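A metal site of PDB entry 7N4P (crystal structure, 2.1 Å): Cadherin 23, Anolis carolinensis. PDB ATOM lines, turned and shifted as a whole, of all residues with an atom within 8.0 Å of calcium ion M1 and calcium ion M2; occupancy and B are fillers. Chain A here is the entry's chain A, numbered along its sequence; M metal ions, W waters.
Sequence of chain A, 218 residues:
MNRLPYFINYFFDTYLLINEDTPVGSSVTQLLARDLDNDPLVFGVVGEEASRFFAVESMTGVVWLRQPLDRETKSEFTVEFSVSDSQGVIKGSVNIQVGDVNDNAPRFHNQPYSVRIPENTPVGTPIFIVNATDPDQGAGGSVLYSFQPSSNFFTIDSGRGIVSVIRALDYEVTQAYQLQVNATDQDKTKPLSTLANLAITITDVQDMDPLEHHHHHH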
ATOM      1  N   GLU A 119      -7.847   5.815  18.041  1.00  0.00           N
ATOM      2  CA  GLU A 119      -8.402   7.183  17.854  1.00  0.00           C
ATOM      3  C   GLU A 119      -9.441   7.471  18.922  1.00  0.00           C
ATOM      4  O   GLU A 119      -9.645   8.625  19.141  1.00  0.00           O
ATOM      5  CB  GLU A 119      -9.042   7.408  16.487  1.00  0.00           C
ATOM      6  CG  GLU A 119     -10.205   6.473  16.209  1.00  0.00           C
ATOM      7  CD  GLU A 119     -10.907   6.735  14.890  1.00  0.00           C
ATOM      8  OE1 GLU A 119     -11.199   7.893  14.598  1.00  0.00           O
ATOM      9  OE2 GLU A 119     -11.158   5.783  14.190  1.00  0.00           O
ATOM     10  N   ASN A 120     -10.109   6.449  19.483  1.00  0.00           N
ATOM     11  CA  ASN A 120     -11.170   6.592  20.514  1.00  0.00           C
ATOM     12  C   ASN A 120     -10.567   6.544  21.920  1.00  0.00           C
ATOM     13  O   ASN A 120     -11.325   6.264  22.839  1.00  0.00           O
ATOM     14  CB  ASN A 120     -12.278   5.544  20.372  1.00  0.00           C
ATOM     15  CG  ASN A 120     -11.860   4.108  20.665  1.00  0.00           C
ATOM     16  OD1 ASN A 120     -10.700   3.717  20.700  1.00  0.00           O
ATOM     17  ND2 ASN A 120     -12.832   3.280  20.941  1.00  0.00           N
ATOM     18  N   LEU A 169      -9.143  12.459  19.678  1.00  0.00           N
ATOM     19  CA  LEU A 169      -8.386  12.173  18.444  1.00  0.00           C
ATOM     20  C   LEU A 169      -9.348  11.796  17.273  1.00  0.00           C
ATOM     21  O   LEU A 169     -10.532  11.582  17.504  1.00  0.00           O
ATOM     22  CB  LEU A 169      -7.451  11.021  18.831  1.00  0.00           C
ATOM     23  CG  LEU A 169      -6.520  11.355  19.987  1.00  0.00           C
ATOM     24  CD1 LEU A 169      -5.727  10.132  20.378  1.00  0.00           C
ATOM     25  CD2 LEU A 169      -5.599  12.500  19.605  1.00  0.00           C
ATOM     26  N   ASP A 170      -8.814  11.660  16.068  1.00  0.00           N
ATOM     27  CA  ASP A 170      -9.585  11.381  14.844  1.00  0.00           C
ATOM     28  C   ASP A 170      -8.629  10.856  13.784  1.00  0.00           C
ATOM     29  O   ASP A 170      -7.972  11.725  13.131  1.00  0.00           O
ATOM     30  CB  ASP A 170     -10.288  12.629  14.338  1.00  0.00           C
ATOM     31  CG  ASP A 170     -11.378  12.317  13.324  1.00  0.00           C
ATOM     32  OD1 ASP A 170     -11.407  11.154  12.795  1.00  0.00           O
ATOM     33  OD2 ASP A 170     -12.175  13.225  13.110  1.00  0.00           O
ATOM     34  N   TYR A 171      -8.628   9.524  13.608  1.00  0.00           N
ATOM     35  CA  TYR A 171      -7.810   8.779  12.611  1.00  0.00           C
ATOM     36  C   TYR A 171      -7.996   9.404  11.235  1.00  0.00           C
ATOM     37  O   TYR A 171      -7.026   9.431  10.480  1.00  0.00           O
ATOM     38  CB  TYR A 171      -8.194   7.300  12.537  1.00  0.00           C
ATOM     39  CG  TYR A 171      -7.380   6.529  11.529  1.00  0.00           C
ATOM     40  CD1 TYR A 171      -6.159   5.970  11.884  1.00  0.00           C
ATOM     41  CD2 TYR A 171      -7.841   6.334  10.220  1.00  0.00           C
ATOM     42  CE1 TYR A 171      -5.416   5.249  10.970  1.00  0.00           C
ATOM     43  CE2 TYR A 171      -7.102   5.611   9.293  1.00  0.00           C
ATOM     44  CZ  TYR A 171      -5.880   5.075   9.667  1.00  0.00           C
ATOM     45  OH  TYR A 171      -5.141   4.385   8.774  1.00  0.00           O
ATOM     46  N   GLU A 172      -9.235   9.846  10.943  1.00  0.00           N
ATOM     47  CA  GLU A 172      -9.657  10.390   9.634  1.00  0.00           C
ATOM     48  C   GLU A 172      -8.995  11.754   9.407  1.00  0.00           C
ATOM     49  O   GLU A 172      -8.739  12.090   8.263  1.00  0.00           O
ATOM     50  CB  GLU A 172     -11.192  10.479   9.525  1.00  0.00           C
ATOM     51  CG  GLU A 172     -11.877   9.158   9.177  1.00  0.00           C
ATOM     52  CD  GLU A 172     -12.008   8.111  10.301  1.00  0.00           C
ATOM     53  OE1 GLU A 172     -12.142   8.503  11.492  1.00  0.00           O
ATOM     54  OE2 GLU A 172     -12.008   6.893   9.986  1.00  0.00           O
ATOM     55  N   VAL A 173      -8.670  12.481  10.466  1.00  0.00           N
ATOM     56  CA  VAL A 173      -7.981  13.790  10.341  1.00  0.00           C
ATOM     57  C   VAL A 173      -6.473  13.571  10.472  1.00  0.00           C
ATOM     58  O   VAL A 173      -5.747  14.132   9.655  1.00  0.00           O
ATOM     59  CB  VAL A 173      -8.517  14.806  11.356  1.00  0.00           C
ATOM     60  CG1 VAL A 173      -7.619  16.023  11.440  1.00  0.00           C
ATOM     61  CG2 VAL A 173      -9.937  15.219  11.002  1.00  0.00           C
ATOM     62  N   ILE A 202      -1.856   6.527  15.469  1.00  0.00           N
ATOM     63  CA  ILE A 202      -3.308   6.465  15.761  1.00  0.00           C
ATOM     64  C   ILE A 202      -3.852   5.298  14.936  1.00  0.00           C
ATOM     65  O   ILE A 202      -3.533   5.249  13.721  1.00  0.00           O
ATOM     66  CB  ILE A 202      -3.981   7.807  15.445  1.00  0.00           C
ATOM     67  CG1 ILE A 202      -3.200   8.964  16.070  1.00  0.00           C
ATOM     68  CG2 ILE A 202      -5.438   7.811  15.860  1.00  0.00           C
ATOM     69  CD1 ILE A 202      -3.305   9.044  17.607  1.00  0.00           C
ATOM     70  N   THR A 203      -4.542   4.358  15.586  1.00  0.00           N
ATOM     71  CA  THR A 203      -5.234   3.213  14.951  1.00  0.00           C
ATOM     72  C   THR A 203      -6.691   3.595  14.651  1.00  0.00           C
ATOM     73  O   THR A 203      -7.365   4.243  15.451  1.00  0.00           O
ATOM     74  CB  THR A 203      -5.069   1.929  15.780  1.00  0.00           C
ATOM     75  OG1 THR A 203      -5.554   2.180  17.099  1.00  0.00           O
ATOM     76  CG2 THR A 203      -3.630   1.476  15.870  1.00  0.00           C
ATOM     77  N   ASP A 204      -7.149   3.244  13.455  1.00  0.00           N
ATOM     78  CA  ASP A 204      -8.540   3.493  13.018  1.00  0.00           C
ATOM     79  C   ASP A 204      -9.492   2.601  13.827  1.00  0.00           C
ATOM     80  O   ASP A 204      -9.190   1.435  14.041  1.00  0.00           O
ATOM     81  CB  ASP A 204      -8.660   3.221  11.533  1.00  0.00           C
ATOM     82  CG  ASP A 204     -10.030   3.477  10.960  1.00  0.00           C
ATOM     83  OD1 ASP A 204     -10.804   4.256  11.526  1.00  0.00           O
ATOM     84  OD2 ASP A 204     -10.297   2.867   9.952  1.00  0.00           O
ATOM     85  N   VAL A 205     -10.631   3.159  14.217  1.00  0.00           N
ATOM     86  CA  VAL A 205     -11.788   2.467  14.836  1.00  0.00           C
ATOM     87  C   VAL A 205     -13.025   2.786  13.986  1.00  0.00           C
ATOM     88  O   VAL A 205     -13.185   3.972  13.593  1.00  0.00           O
ATOM     89  CB  VAL A 205     -11.976   2.999  16.271  1.00  0.00           C
ATOM     90  CG1 VAL A 205     -13.377   2.727  16.785  1.00  0.00           C
ATOM     91  CG2 VAL A 205     -10.903   2.466  17.199  1.00  0.00           C
ATOM     92  N   GLN A 206     -13.886   1.803  13.775  1.00  0.00           N
ATOM     93  CA  GLN A 206     -15.162   1.973  13.036  1.00  0.00           C
ATOM     94  C   GLN A 206     -16.089   2.847  13.862  1.00  0.00           C
ATOM     95  O   GLN A 206     -16.248   2.512  15.041  1.00  0.00           O
ATOM     96  CB  GLN A 206     -15.829   0.619  12.851  1.00  0.00           C
ATOM     97  CG  GLN A 206     -15.037  -0.327  11.974  1.00  0.00           C
ATOM     98  CD  GLN A 206     -15.801  -1.579  11.623  1.00  0.00           C
ATOM     99  OE1 GLN A 206     -16.929  -1.817  12.056  1.00  0.00           O
ATOM    100  NE2 GLN A 206     -15.183  -2.433  10.818  1.00  0.00           N
ATOM    101  N   ASP A 207     -16.669   3.909  13.288  1.00  0.00           N
ATOM    102  CA  ASP A 207     -17.738   4.736  13.934  1.00  0.00           C
ATOM    103  C   ASP A 207     -19.104   4.422  13.293  1.00  0.00           C
ATOM    104  O   ASP A 207     -19.762   3.455  13.664  1.00  0.00           O
ATOM    105  CB  ASP A 207     -17.429   6.244  13.858  1.00  0.00           C
ATOM    106  CG  ASP A 207     -17.301   6.793  12.443  1.00  0.00           C
ATOM    107  OD1 ASP A 207     -18.203   6.500  11.603  1.00  0.00           O
ATOM    108  OD2 ASP A 207     -16.276   7.486  12.170  1.00  0.00           O
HETATM  109 CA    CA M   1     -12.932   9.164  13.622  1.00  0.00          CA
HETATM  110 CA    CA M   2     -12.653   5.686  12.180  1.00  0.00          CA
HETATM  111  O   HOH W   1     -14.321   6.358  13.678  1.00  0.00           O
HETATM  112  O   HOH W   2     -14.296   4.367  11.235  1.00  0.00           O
HETATM  113  O   HOH W   3     -14.729   9.863  12.834  1.00  0.00           O
HETATM  114  O   HOH W   4     -13.284  10.421  15.450  1.00  0.00           O
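OE1 of Glu 119 sits close to N of Tyr 171, 3.2 Å away. N of Glu 119 lies within hydrogen-bond range of O of Thr 203, at 3.1 Å.
Three residues have an atom within 4 Å of calcium ion M1: Glu 119, Asp 170 and Glu 172.
Calcium ion M2 is bound by the backbone carbonyl oxygen of Val 205, water W2, water W1, the side-chain carboxylate of Asp 204, the side-chain carboxylate of Glu 119 and the side-chain carboxylate of Glu 172. Slightly farther from calcium ion M2 lies OE1 of Glu 172 (2.9 Å).
Of the 13 residues printed, 4 come within 4 Å of calcium ion M2. Along chain A the residues within 4 Å of calcium ion M2 span positions 119 to 205.
Calcium ion M1 is bound by water W3 (2.1 Å), water W4 (2.2 Å), OE1 of Glu 119 (2.4 Å), OE1 of Glu 172 (2.4 Å) and OD1 of Asp 170 (2.6 Å). Slightly farther from calcium ion M1 lies water W1 (3.1 Å).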
